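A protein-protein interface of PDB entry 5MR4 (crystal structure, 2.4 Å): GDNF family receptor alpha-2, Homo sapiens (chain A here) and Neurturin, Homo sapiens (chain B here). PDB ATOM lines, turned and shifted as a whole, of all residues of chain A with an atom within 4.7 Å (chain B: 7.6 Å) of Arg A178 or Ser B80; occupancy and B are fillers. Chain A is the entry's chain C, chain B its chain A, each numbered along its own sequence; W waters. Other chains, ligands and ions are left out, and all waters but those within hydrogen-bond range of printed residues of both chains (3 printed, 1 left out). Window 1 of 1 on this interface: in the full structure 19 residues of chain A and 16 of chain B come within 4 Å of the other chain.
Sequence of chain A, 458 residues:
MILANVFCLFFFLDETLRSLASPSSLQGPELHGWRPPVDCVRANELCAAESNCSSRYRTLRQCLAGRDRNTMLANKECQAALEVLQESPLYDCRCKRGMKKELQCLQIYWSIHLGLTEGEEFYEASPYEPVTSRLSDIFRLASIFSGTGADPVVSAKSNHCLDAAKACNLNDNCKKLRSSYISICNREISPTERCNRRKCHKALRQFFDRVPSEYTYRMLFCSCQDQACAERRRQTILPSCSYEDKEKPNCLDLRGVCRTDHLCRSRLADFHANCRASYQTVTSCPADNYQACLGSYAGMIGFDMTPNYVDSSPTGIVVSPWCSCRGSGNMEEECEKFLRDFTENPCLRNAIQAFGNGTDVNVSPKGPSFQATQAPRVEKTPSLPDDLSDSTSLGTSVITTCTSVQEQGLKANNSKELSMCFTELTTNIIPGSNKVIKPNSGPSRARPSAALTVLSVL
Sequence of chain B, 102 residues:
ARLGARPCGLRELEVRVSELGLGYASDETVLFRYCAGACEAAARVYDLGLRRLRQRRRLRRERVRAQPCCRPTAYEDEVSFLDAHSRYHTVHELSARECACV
The side-chain carboxylate (OE1) of Glu B28 sits at hydrogen-bond distance from the side-chain amide nitrogen (ND2) of Asn A169, at 3.4 Å. The side-chain carboxylate (OE1) of Glu B28 lies within salt-bridge range of the guanidinium group (NH1) of Arg A178, at 2.8 Å. OE2 of Glu B28 is in salt-bridge range of NH1 of Arg A232, at 2.8 Å. The side-chain amide nitrogen (ND2) of Asn A169 sits at hydrogen-bond distance from the backbone carbonyl oxygen (O) of Thr B29, at 3.3 Å. The side-chain amino group of Lys A175 lies within salt-bridge range of the side-chain carboxylate of Glu B76, at 2.8 Å. OE1 of Glu B78 lies within hydrogen-bond range of OG of Ser A179, at 2.8 Å. OG of Ser A183 sits at hydrogen-bond distance from OE1 of Glu B78 (3.1 Å). ND2 of Asn A169 sits at hydrogen-bond distance from O of Ser B80 (3.2 Å). O of Ser B80 lies within hydrogen-bond range of NH1 of Arg A178 (3.4 Å). OG of Ser A179 is in hydrogen-bond range of OG of Ser B80 (2.7 Å). The backbone carbonyl oxygen (O) of Leu B82 sits at hydrogen-bond distance from the guanidinium group (NH2) of Arg A232, 3.0 Å away.
O of Glu B28 sits at hydrogen-bond distance from N of Val B17 (2.9 Å). The side-chain hydroxyl of Ser B26 sits at hydrogen-bond distance from the backbone NH of Glu B28. OE2 of Glu B28 lies within hydrogen-bond range of N of Leu B82, at 2.8 Å. O of His B89 lies close to OG of Ser B80 (3.5 Å). The guanidinium group (NH1) of Arg A178 lies within hydrogen-bond range of the side-chain amide oxygen (OD1) of Asn A169 (3.2 Å). The backbone carbonyl oxygen (O) of Ser A180 lies within hydrogen-bond range of the side-chain hydroxyl (OG) of Ser A183, at 3.2 Å.
Glu B28 touches Ala A165 (OE1 to CB, 3.8 Å). CG1 of Val B30 touches ND2 of Asn A169, 3.9 Å away. Lys A175 touches Glu B78. CG2 of Val B79 touches CG of Lys A175 (3.97 Å). Val B79 touches Ser A179 (C to OG, 3.5 Å). Thr B90 touches Ser A179. Ser A180 touches Glu B78 (N to OE1, 3.5 Å). OG of Ser B80 touches CG2 of Ile A182 (3.7 Å). Tyr B88 touches Ile A182 (CE1 to CD1, 3.6 Å). CB of Ser A183 touches OG1 of Thr B90, 3.5 Å away.
Of the printed residues of chain B, Arg A178 touches Glu B28 and Ser B80. Printed residues of chain A within 4 Å of Glu B28: Ala A165 (3.8 Å), Asn A169 (3.4 Å), Arg A178 (2.8 Å) and Arg A232 (2.8 Å). Of the printed residues of chain A, Val B79 touches Lys A175 and Ser A179. Ser B80 touches four residues of chain A.
Printed residues of chain B that touch a printed residue of chain A: Glu B28, Thr B29, Val B30, Glu B76, Glu B78, Val B79, Ser B80, Leu B82, Tyr B88 and Thr B90. Hydrophobic or aromatic side chains of chain A that line the printed part of chain B: Ala A165 and Ile A182. Among the printed residues, 21 pairs touch across the chains. Among the printed residues, Asp or Glu carboxylates within 4 Å of a Lys or Arg side-chain nitrogen of the other chain: Lys A175 with Glu B76 (2.8 Å), Arg A178 with Glu B28 (2.8 Å) and Arg A232 with Glu B28 (2.8 Å).
Water W3 bridges OH of Tyr B88 (2.8 Å) and O of Arg A232 (2.8 Å). Water W1 lies within hydrogen-bond range of the side-chain amide oxygen (OD1) of Asn A169 (2.8 Å), the backbone carbonyl oxygen (O) of Lys A175 (3.1 Å) and the backbone NH (N) of Ser B80 (3.1 Å). Water W2 lies within hydrogen-bond range of the side-chain hydroxyl (OH) of Tyr A181, the guanidinium group (NE) of Arg A178 and the side-chain hydroxyl (OH) of Tyr B88.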
ATOM      1  N   ALA A 165     -19.371   7.592   6.612  1.00  0.00           N
ATOM      2  CA  ALA A 165     -18.781   8.790   5.991  1.00  0.00           C
ATOM      3  C   ALA A 165     -18.711   9.957   6.968  1.00  0.00           C
ATOM      4  O   ALA A 165     -17.760  10.734   6.928  1.00  0.00           O
ATOM      5  CB  ALA A 165     -19.570   9.198   4.772  1.00  0.00           C
ATOM      6  N   CYS A 168     -15.871   9.397   9.434  1.00  0.00           N
ATOM      7  CA  CYS A 168     -14.623   9.652   8.726  1.00  0.00           C
ATOM      8  C   CYS A 168     -14.331  11.143   8.585  1.00  0.00           C
ATOM      9  O   CYS A 168     -13.241  11.594   8.912  1.00  0.00           O
ATOM     10  CB  CYS A 168     -14.662   9.008   7.351  1.00  0.00           C
ATOM     11  SG  CYS A 168     -13.166   9.294   6.413  1.00  0.00           S
ATOM     12  N   ASN A 169     -15.311  11.905   8.105  1.00  0.00           N
ATOM     13  CA  ASN A 169     -15.165  13.360   7.971  1.00  0.00           C
ATOM     14  C   ASN A 169     -15.002  14.107   9.297  1.00  0.00           C
ATOM     15  O   ASN A 169     -14.517  15.244   9.290  1.00  0.00           O
ATOM     16  CB  ASN A 169     -16.323  13.997   7.161  1.00  0.00           C
ATOM     17  CG  ASN A 169     -16.088  13.983   5.646  1.00  0.00           C
ATOM     18  OD1 ASN A 169     -15.104  13.447   5.129  1.00  0.00           O
ATOM     19  ND2 ASN A 169     -17.016  14.576   4.926  1.00  0.00           N
ATOM     20  N   CYS A 174      -8.738  10.724   8.766  1.00  0.00           N
ATOM     21  CA  CYS A 174      -9.622  10.042   7.816  1.00  0.00           C
ATOM     22  C   CYS A 174     -10.119  11.043   6.777  1.00  0.00           C
ATOM     23  O   CYS A 174     -10.055  10.762   5.597  1.00  0.00           O
ATOM     24  CB  CYS A 174     -10.823   9.359   8.501  1.00  0.00           C
ATOM     25  SG  CYS A 174     -11.715   8.185   7.419  1.00  0.00           S
ATOM     26  N   LYS A 175     -10.554  12.217   7.239  1.00  0.00           N
ATOM     27  CA  LYS A 175     -11.060  13.263   6.364  1.00  0.00           C
ATOM     28  C   LYS A 175     -10.052  13.704   5.344  1.00  0.00           C
ATOM     29  O   LYS A 175     -10.403  13.878   4.178  1.00  0.00           O
ATOM     30  CB  LYS A 175     -11.512  14.479   7.186  1.00  0.00           C
ATOM     31  CG  LYS A 175     -12.077  15.635   6.368  1.00  0.00           C
ATOM     32  CD  LYS A 175     -11.682  16.979   6.951  1.00  0.00           C
ATOM     33  CE  LYS A 175     -10.259  17.357   6.609  1.00  0.00           C
ATOM     34  NZ  LYS A 175      -9.885  18.490   7.478  1.00  0.00           N
ATOM     35  N   LYS A 176      -8.820  13.921   5.781  1.00  0.00           N
ATOM     36  CA  LYS A 176      -7.728  14.297   4.879  1.00  0.00           C
ATOM     37  C   LYS A 176      -7.461  13.228   3.811  1.00  0.00           C
ATOM     38  O   LYS A 176      -7.430  13.530   2.640  1.00  0.00           O
ATOM     39  CB  LYS A 176      -6.412  14.520   5.651  1.00  0.00           C
ATOM     40  CG  LYS A 176      -6.315  15.867   6.368  1.00  0.00           C
ATOM     41  CD  LYS A 176      -5.115  15.988   7.319  1.00  0.00           C
ATOM     42  CE  LYS A 176      -5.087  17.333   8.055  1.00  0.00           C
ATOM     43  NZ  LYS A 176      -6.252  17.548   8.973  1.00  0.00           N
ATOM     44  N   LEU A 177      -7.225  11.996   4.243  1.00  0.00           N
ATOM     45  CA  LEU A 177      -6.816  10.922   3.349  1.00  0.00           C
ATOM     46  C   LEU A 177      -7.995  10.454   2.451  1.00  0.00           C
ATOM     47  O   LEU A 177      -7.770  10.053   1.310  1.00  0.00           O
ATOM     48  CB  LEU A 177      -6.191   9.774   4.140  1.00  0.00           C
ATOM     49  CG  LEU A 177      -4.690   9.914   4.476  1.00  0.00           C
ATOM     50  CD1 LEU A 177      -4.371  11.174   5.251  1.00  0.00           C
ATOM     51  CD2 LEU A 177      -4.266   8.738   5.333  1.00  0.00           C
ATOM     52  N   ARG A 178      -9.231  10.577   2.956  1.00  0.00           N
ATOM     53  CA  ARG A 178     -10.416  10.363   2.160  1.00  0.00           C
ATOM     54  C   ARG A 178     -10.518  11.402   1.051  1.00  0.00           C
ATOM     55  O   ARG A 178     -10.653  11.064  -0.140  1.00  0.00           O
ATOM     56  CB  ARG A 178     -11.673  10.426   3.024  1.00  0.00           C
ATOM     57  CG  ARG A 178     -12.901   9.883   2.325  1.00  0.00           C
ATOM     58  CD  ARG A 178     -14.158  10.525   2.843  1.00  0.00           C
ATOM     59  NE  ARG A 178     -15.333  10.081   2.103  1.00  0.00           N
ATOM     60  CZ  ARG A 178     -16.537  10.624   2.212  1.00  0.00           C
ATOM     61  NH1 ARG A 178     -16.763  11.648   3.034  1.00  0.00           N
ATOM     62  NH2 ARG A 178     -17.537  10.130   1.502  1.00  0.00           N
ATOM     63  N   SER A 179     -10.459  12.667   1.442  1.00  0.00           N
ATOM     64  CA  SER A 179     -10.555  13.735   0.466  1.00  0.00           C
ATOM     65  C   SER A 179      -9.430  13.672  -0.549  1.00  0.00           C
ATOM     66  O   SER A 179      -9.612  14.002  -1.706  1.00  0.00           O
ATOM     67  CB  SER A 179     -10.538  15.110   1.144  1.00  0.00           C
ATOM     68  OG  SER A 179     -10.890  16.091   0.213  1.00  0.00           O
ATOM     69  N   SER A 180      -8.257  13.264  -0.108  1.00  0.00           N
ATOM     70  CA  SER A 180      -7.134  13.174  -1.007  1.00  0.00           C
ATOM     71  C   SER A 180      -7.377  12.148  -2.146  1.00  0.00           C
ATOM     72  O   SER A 180      -7.120  12.457  -3.298  1.00  0.00           O
ATOM     73  CB  SER A 180      -5.871  12.858  -0.205  1.00  0.00           C
ATOM     74  OG  SER A 180      -4.831  12.482  -1.090  1.00  0.00           O
ATOM     75  N   TYR A 181      -7.877  10.948  -1.835  1.00  0.00           N
ATOM     76  CA  TYR A 181      -8.127   9.954  -2.897  1.00  0.00           C
ATOM     77  C   TYR A 181      -9.352  10.332  -3.712  1.00  0.00           C
ATOM     78  O   TYR A 181      -9.400  10.072  -4.916  1.00  0.00           O
ATOM     79  CB  TYR A 181      -8.195   8.509  -2.359  1.00  0.00           C
ATOM     80  CG  TYR A 181      -9.511   7.987  -1.823  1.00  0.00           C
ATOM     81  CD1 TYR A 181     -10.570   7.676  -2.667  1.00  0.00           C
ATOM     82  CD2 TYR A 181      -9.680   7.743  -0.472  1.00  0.00           C
ATOM     83  CE1 TYR A 181     -11.774   7.204  -2.170  1.00  0.00           C
ATOM     84  CE2 TYR A 181     -10.878   7.258   0.024  1.00  0.00           C
ATOM     85  CZ  TYR A 181     -11.929   6.982  -0.838  1.00  0.00           C
ATOM     86  OH  TYR A 181     -13.117   6.448  -0.321  1.00  0.00           O
ATOM     87  N   ILE A 182     -10.344  10.959  -3.071  1.00  0.00           N
ATOM     88  CA  ILE A 182     -11.508  11.394  -3.803  1.00  0.00           C
ATOM     89  C   ILE A 182     -11.115  12.418  -4.860  1.00  0.00           C
ATOM     90  O   ILE A 182     -11.467  12.270  -6.041  1.00  0.00           O
ATOM     91  CB  ILE A 182     -12.630  11.924  -2.889  1.00  0.00           C
ATOM     92  CG1 ILE A 182     -13.322  10.741  -2.215  1.00  0.00           C
ATOM     93  CG2 ILE A 182     -13.678  12.653  -3.713  1.00  0.00           C
ATOM     94  CD1 ILE A 182     -14.088  11.107  -0.977  1.00  0.00           C
ATOM     95  N   SER A 183     -10.341  13.417  -4.462  1.00  0.00           N
ATOM     96  CA  SER A 183     -10.020  14.508  -5.385  1.00  0.00           C
ATOM     97  C   SER A 183      -9.082  14.059  -6.484  1.00  0.00           C
ATOM     98  O   SER A 183      -9.217  14.502  -7.600  1.00  0.00           O
ATOM     99  CB  SER A 183      -9.441  15.719  -4.654  1.00  0.00           C
ATOM    100  OG  SER A 183      -8.291  15.359  -3.962  1.00  0.00           O
ATOM    101  N   PHE A 207      -5.027   5.478   1.846  1.00  0.00           N
ATOM    102  CA  PHE A 207      -6.231   5.534   2.708  1.00  0.00           C
ATOM    103  C   PHE A 207      -6.382   4.234   3.502  1.00  0.00           C
ATOM    104  O   PHE A 207      -6.562   4.250   4.714  1.00  0.00           O
ATOM    105  CB  PHE A 207      -7.471   5.809   1.844  1.00  0.00           C
ATOM    106  CG  PHE A 207      -8.762   5.834   2.596  1.00  0.00           C
ATOM    107  CD1 PHE A 207      -9.093   6.905   3.406  1.00  0.00           C
ATOM    108  CD2 PHE A 207      -9.679   4.794   2.464  1.00  0.00           C
ATOM    109  CE1 PHE A 207     -10.292   6.942   4.068  1.00  0.00           C
ATOM    110  CE2 PHE A 207     -10.883   4.836   3.128  1.00  0.00           C
ATOM    111  CZ  PHE A 207     -11.179   5.902   3.936  1.00  0.00           C
ATOM    112  N   MET A 219     -16.819   1.967   6.177  1.00  0.00           N
ATOM    113  CA  MET A 219     -17.194   2.515   4.873  1.00  0.00           C
ATOM    114  C   MET A 219     -17.301   1.449   3.762  1.00  0.00           C
ATOM    115  O   MET A 219     -18.243   1.476   2.965  1.00  0.00           O
ATOM    116  CB  MET A 219     -16.200   3.578   4.441  1.00  0.00           C
ATOM    117  CG  MET A 219     -16.159   4.763   5.391  1.00  0.00           C
ATOM    118  SD  MET A 219     -14.962   6.031   4.973  1.00  0.00           S
ATOM    119  CE  MET A 219     -15.603   6.571   3.399  1.00  0.00           C
ATOM    120  N   ARG A 232     -23.913   4.275  -2.405  1.00  0.00           N
ATOM    121  CA  ARG A 232     -22.882   4.953  -1.659  1.00  0.00           C
ATOM    122  C   ARG A 232     -21.720   3.971  -1.362  1.00  0.00           C
ATOM    123  O   ARG A 232     -20.574   4.282  -1.631  1.00  0.00           O
ATOM    124  CB  ARG A 232     -23.455   5.579  -0.408  1.00  0.00           C
ATOM    125  CG  ARG A 232     -22.415   6.196   0.493  1.00  0.00           C
ATOM    126  CD  ARG A 232     -23.097   6.939   1.625  1.00  0.00           C
ATOM    127  NE  ARG A 232     -23.638   8.216   1.187  1.00  0.00           N
ATOM    128  CZ  ARG A 232     -22.922   9.337   1.087  1.00  0.00           C
ATOM    129  NH1 ARG A 232     -21.617   9.347   1.362  1.00  0.00           N
ATOM    130  NH2 ARG A 232     -23.496  10.457   0.681  1.00  0.00           N
ATOM    131  N   VAL B  17     -23.798  19.335   4.646  1.00  0.00           N
ATOM    132  CA  VAL B  17     -23.284  20.182   3.565  1.00  0.00           C
ATOM    133  C   VAL B  17     -24.411  20.880   2.760  1.00  0.00           C
ATOM    134  O   VAL B  17     -24.177  21.956   2.205  1.00  0.00           O
ATOM    135  CB  VAL B  17     -22.260  19.499   2.592  1.00  0.00           C
ATOM    136  CG1 VAL B  17     -21.270  18.582   3.304  1.00  0.00           C
ATOM    137  CG2 VAL B  17     -22.950  18.721   1.519  1.00  0.00           C
ATOM    138  N   SER B  26     -26.228  17.215  -0.812  1.00  0.00           N
ATOM    139  CA  SER B  26     -25.691  16.050  -0.099  1.00  0.00           C
ATOM    140  C   SER B  26     -26.098  15.989   1.351  1.00  0.00           C
ATOM    141  O   SER B  26     -26.119  17.011   2.040  1.00  0.00           O
ATOM    142  CB  SER B  26     -24.167  16.076  -0.173  1.00  0.00           C
ATOM    143  OG  SER B  26     -23.604  15.032   0.599  1.00  0.00           O
ATOM    144  N   GLU B  28     -24.209  14.402   3.505  1.00  0.00           N
ATOM    145  CA  GLU B  28     -22.998  14.250   4.279  1.00  0.00           C
ATOM    146  C   GLU B  28     -22.827  15.382   5.292  1.00  0.00           C
ATOM    147  O   GLU B  28     -23.392  16.470   5.129  1.00  0.00           O
ATOM    148  CB  GLU B  28     -21.775  14.141   3.380  1.00  0.00           C
ATOM    149  CG  GLU B  28     -21.669  12.777   2.690  1.00  0.00           C
ATOM    150  CD  GLU B  28     -20.240  12.312   2.488  1.00  0.00           C
ATOM    151  OE1 GLU B  28     -19.356  12.676   3.341  1.00  0.00           O
ATOM    152  OE2 GLU B  28     -20.001  11.603   1.456  1.00  0.00           O
ATOM    153  N   THR B  29     -22.082  15.072   6.349  1.00  0.00           N
ATOM    154  CA  THR B  29     -21.735  16.009   7.405  1.00  0.00           C
ATOM    155  C   THR B  29     -20.265  16.430   7.248  1.00  0.00           C
ATOM    156  O   THR B  29     -19.427  15.620   6.861  1.00  0.00           O
ATOM    157  CB  THR B  29     -21.962  15.338   8.784  1.00  0.00           C
ATOM    158  OG1 THR B  29     -23.335  15.005   8.888  1.00  0.00           O
ATOM    159  CG2 THR B  29     -21.606  16.246   9.994  1.00  0.00           C
ATOM    160  N   VAL B  30     -19.966  17.693   7.540  1.00  0.00           N
ATOM    161  CA  VAL B  30     -18.583  18.143   7.726  1.00  0.00           C
ATOM    162  C   VAL B  30     -18.439  18.821   9.074  1.00  0.00           C
ATOM    163  O   VAL B  30     -19.418  19.310   9.661  1.00  0.00           O
ATOM    164  CB  VAL B  30     -18.083  19.082   6.604  1.00  0.00           C
ATOM    165  CG1 VAL B  30     -18.043  18.355   5.272  1.00  0.00           C
ATOM    166  CG2 VAL B  30     -18.944  20.324   6.471  1.00  0.00           C
ATOM    167  N   GLU B  76      -8.534  25.245   6.030  1.00  0.00           N
ATOM    168  CA  GLU B  76      -8.529  23.811   5.684  1.00  0.00           C
ATOM    169  C   GLU B  76      -8.183  23.591   4.215  1.00  0.00           C
ATOM    170  O   GLU B  76      -8.672  24.320   3.379  1.00  0.00           O
ATOM    171  CB  GLU B  76      -9.921  23.230   5.992  1.00  0.00           C
ATOM    172  CG  GLU B  76     -10.234  21.861   5.416  1.00  0.00           C
ATOM    173  CD  GLU B  76     -11.643  21.375   5.794  1.00  0.00           C
ATOM    174  OE1 GLU B  76     -11.770  20.432   6.599  1.00  0.00           O
ATOM    175  OE2 GLU B  76     -12.626  21.930   5.302  1.00  0.00           O
ATOM    176  N   GLU B  78      -8.807  20.825   2.127  1.00  0.00           N
ATOM    177  CA  GLU B  78      -9.916  20.249   1.367  1.00  0.00           C
ATOM    178  C   GLU B  78     -10.782  19.307   2.174  1.00  0.00           C
ATOM    179  O   GLU B  78     -10.319  18.666   3.109  1.00  0.00           O
ATOM    180  CB  GLU B  78      -9.408  19.519   0.107  1.00  0.00           C
ATOM    181  CG  GLU B  78      -8.275  18.519   0.322  1.00  0.00           C
ATOM    182  CD  GLU B  78      -7.957  17.753  -0.969  1.00  0.00           C
ATOM    183  OE1 GLU B  78      -8.492  16.635  -1.152  1.00  0.00           O
ATOM    184  OE2 GLU B  78      -7.224  18.301  -1.836  1.00  0.00           O
ATOM    185  N   VAL B  79     -12.051  19.233   1.791  1.00  0.00           N
ATOM    186  CA  VAL B  79     -12.976  18.235   2.316  1.00  0.00           C
ATOM    187  C   VAL B  79     -13.809  17.718   1.129  1.00  0.00           C
ATOM    188  O   VAL B  79     -14.088  18.443   0.175  1.00  0.00           O
ATOM    189  CB  VAL B  79     -13.825  18.814   3.475  1.00  0.00           C
ATOM    190  CG1 VAL B  79     -14.756  19.918   3.005  1.00  0.00           C
ATOM    191  CG2 VAL B  79     -14.628  17.722   4.160  1.00  0.00           C
ATOM    192  N   SER B  80     -14.193  16.460   1.181  1.00  0.00           N
ATOM    193  CA  SER B  80     -14.943  15.857   0.087  1.00  0.00           C
ATOM    194  C   SER B  80     -16.177  15.138   0.607  1.00  0.00           C
ATOM    195  O   SER B  80     -16.273  14.782   1.789  1.00  0.00           O
ATOM    196  CB  SER B  80     -14.069  14.871  -0.699  1.00  0.00           C
ATOM    197  OG  SER B  80     -13.015  15.508  -1.416  1.00  0.00           O
ATOM    198  N   PHE B  81     -17.100  14.875  -0.306  1.00  0.00           N
ATOM    199  CA  PHE B  81     -18.329  14.180   0.020  1.00  0.00           C
ATOM    200  C   PHE B  81     -19.025  13.710  -1.264  1.00  0.00           C
ATOM    201  O   PHE B  81     -18.760  14.221  -2.348  1.00  0.00           O
ATOM    202  CB  PHE B  81     -19.269  15.118   0.817  1.00  0.00           C
ATOM    203  CG  PHE B  81     -19.414  16.487   0.204  1.00  0.00           C
ATOM    204  CD1 PHE B  81     -20.311  16.711  -0.825  1.00  0.00           C
ATOM    205  CD2 PHE B  81     -18.635  17.547   0.642  1.00  0.00           C
ATOM    206  CE1 PHE B  81     -20.437  17.956  -1.406  1.00  0.00           C
ATOM    207  CE2 PHE B  81     -18.767  18.818   0.068  1.00  0.00           C
ATOM    208  CZ  PHE B  81     -19.661  19.012  -0.965  1.00  0.00           C
ATOM    209  N   LEU B  82     -19.934  12.753  -1.110  1.00  0.00           N
ATOM    210  CA  LEU B  82     -20.712  12.227  -2.207  1.00  0.00           C
ATOM    211  C   LEU B  82     -22.115  12.831  -2.083  1.00  0.00           C
ATOM    212  O   LEU B  82     -22.681  12.870  -0.981  1.00  0.00           O
ATOM    213  CB  LEU B  82     -20.757  10.699  -2.124  1.00  0.00           C
ATOM    214  CG  LEU B  82     -21.508   9.971  -3.254  1.00  0.00           C
ATOM    215  CD1 LEU B  82     -20.679   9.873  -4.508  1.00  0.00           C
ATOM    216  CD2 LEU B  82     -21.878   8.585  -2.782  1.00  0.00           C
ATOM    217  N   TYR B  88     -19.195  12.832  -6.583  1.00  0.00           N
ATOM    218  CA  TYR B  88     -18.280  13.276  -5.546  1.00  0.00           C
ATOM    219  C   TYR B  88     -17.924  14.743  -5.753  1.00  0.00           C
ATOM    220  O   TYR B  88     -17.831  15.185  -6.869  1.00  0.00           O
ATOM    221  CB  TYR B  88     -16.995  12.433  -5.559  1.00  0.00           C
ATOM    222  CG  TYR B  88     -17.047  11.167  -4.740  1.00  0.00           C
ATOM    223  CD1 TYR B  88     -17.086  11.212  -3.352  1.00  0.00           C
ATOM    224  CD2 TYR B  88     -17.014   9.912  -5.352  1.00  0.00           C
ATOM    225  CE1 TYR B  88     -17.106  10.054  -2.586  1.00  0.00           C
ATOM    226  CE2 TYR B  88     -17.022   8.756  -4.589  1.00  0.00           C
ATOM    227  CZ  TYR B  88     -17.072   8.823  -3.203  1.00  0.00           C
ATOM    228  OH  TYR B  88     -17.088   7.637  -2.442  1.00  0.00           O
ATOM    229  N   HIS B  89     -17.717  15.477  -4.659  1.00  0.00           N
ATOM    230  CA  HIS B  89     -17.227  16.869  -4.716  1.00  0.00           C
ATOM    231  C   HIS B  89     -16.138  17.086  -3.695  1.00  0.00           C
ATOM    232  O   HIS B  89     -16.127  16.425  -2.678  1.00  0.00           O
ATOM    233  CB  HIS B  89     -18.357  17.842  -4.457  1.00  0.00           C
ATOM    234  CG  HIS B  89     -19.533  17.641  -5.358  1.00  0.00           C
ATOM    235  ND1 HIS B  89     -19.653  18.270  -6.577  1.00  0.00           N
ATOM    236  CD2 HIS B  89     -20.651  16.891  -5.211  1.00  0.00           C
ATOM    237  CE1 HIS B  89     -20.788  17.908  -7.149  1.00  0.00           C
ATOM    238  NE2 HIS B  89     -21.420  17.083  -6.332  1.00  0.00           N
ATOM    239  N   THR B  90     -15.187  17.951  -4.037  1.00  0.00           N
ATOM    240  CA  THR B  90     -14.134  18.406  -3.146  1.00  0.00           C
ATOM    241  C   THR B  90     -14.209  19.923  -3.013  1.00  0.00           C
ATOM    242  O   THR B  90     -14.243  20.597  -4.020  1.00  0.00           O
ATOM    243  CB  THR B  90     -12.756  18.052  -3.666  1.00  0.00           C
ATOM    244  OG1 THR B  90     -12.695  16.652  -3.860  1.00  0.00           O
ATOM    245  CG2 THR B  90     -11.698  18.429  -2.628  1.00  0.00           C
ATOM    246  N   VAL B  91     -14.239  20.430  -1.775  1.00  0.00           N
ATOM    247  CA  VAL B  91     -14.278  21.870  -1.501  1.00  0.00           C
ATOM    248  C   VAL B  91     -12.994  22.275  -0.807  1.00  0.00           C
ATOM    249  O   VAL B  91     -12.576  21.656   0.162  1.00  0.00           O
ATOM    250  CB  VAL B  91     -15.488  22.268  -0.646  1.00  0.00           C
ATOM    251  CG1 VAL B  91     -15.587  23.782  -0.533  1.00  0.00           C
ATOM    252  CG2 VAL B  91     -16.757  21.777  -1.314  1.00  0.00           C
ATOM    253  N   HIS B  92     -12.380  23.324  -1.321  1.00  0.00           N
ATOM    254  CA  HIS B  92     -11.137  23.875  -0.778  1.00  0.00           C
ATOM    255  C   HIS B  92     -11.431  25.066   0.127  1.00  0.00           C
ATOM    256  O   HIS B  92     -12.295  25.886  -0.184  1.00  0.00           O
ATOM    257  CB  HIS B  92     -10.191  24.266  -1.916  1.00  0.00           C
ATOM    258  CG  HIS B  92      -9.880  23.129  -2.831  1.00  0.00           C
ATOM    259  ND1 HIS B  92      -8.767  22.329  -2.677  1.00  0.00           N
ATOM    260  CD2 HIS B  92     -10.569  22.622  -3.885  1.00  0.00           C
ATOM    261  CE1 HIS B  92      -8.779  21.383  -3.603  1.00  0.00           C
ATOM    262  NE2 HIS B  92      -9.858  21.544  -4.350  1.00  0.00           N
HETATM  263  O   HOH W   1     -13.270  14.202   3.138  1.00  0.00           O
HETATM  264  O   HOH W   2     -15.583   7.777   0.351  1.00  0.00           O
HETATM  265  O   HOH W   3     -19.068   6.504  -0.851  1.00  0.00           O
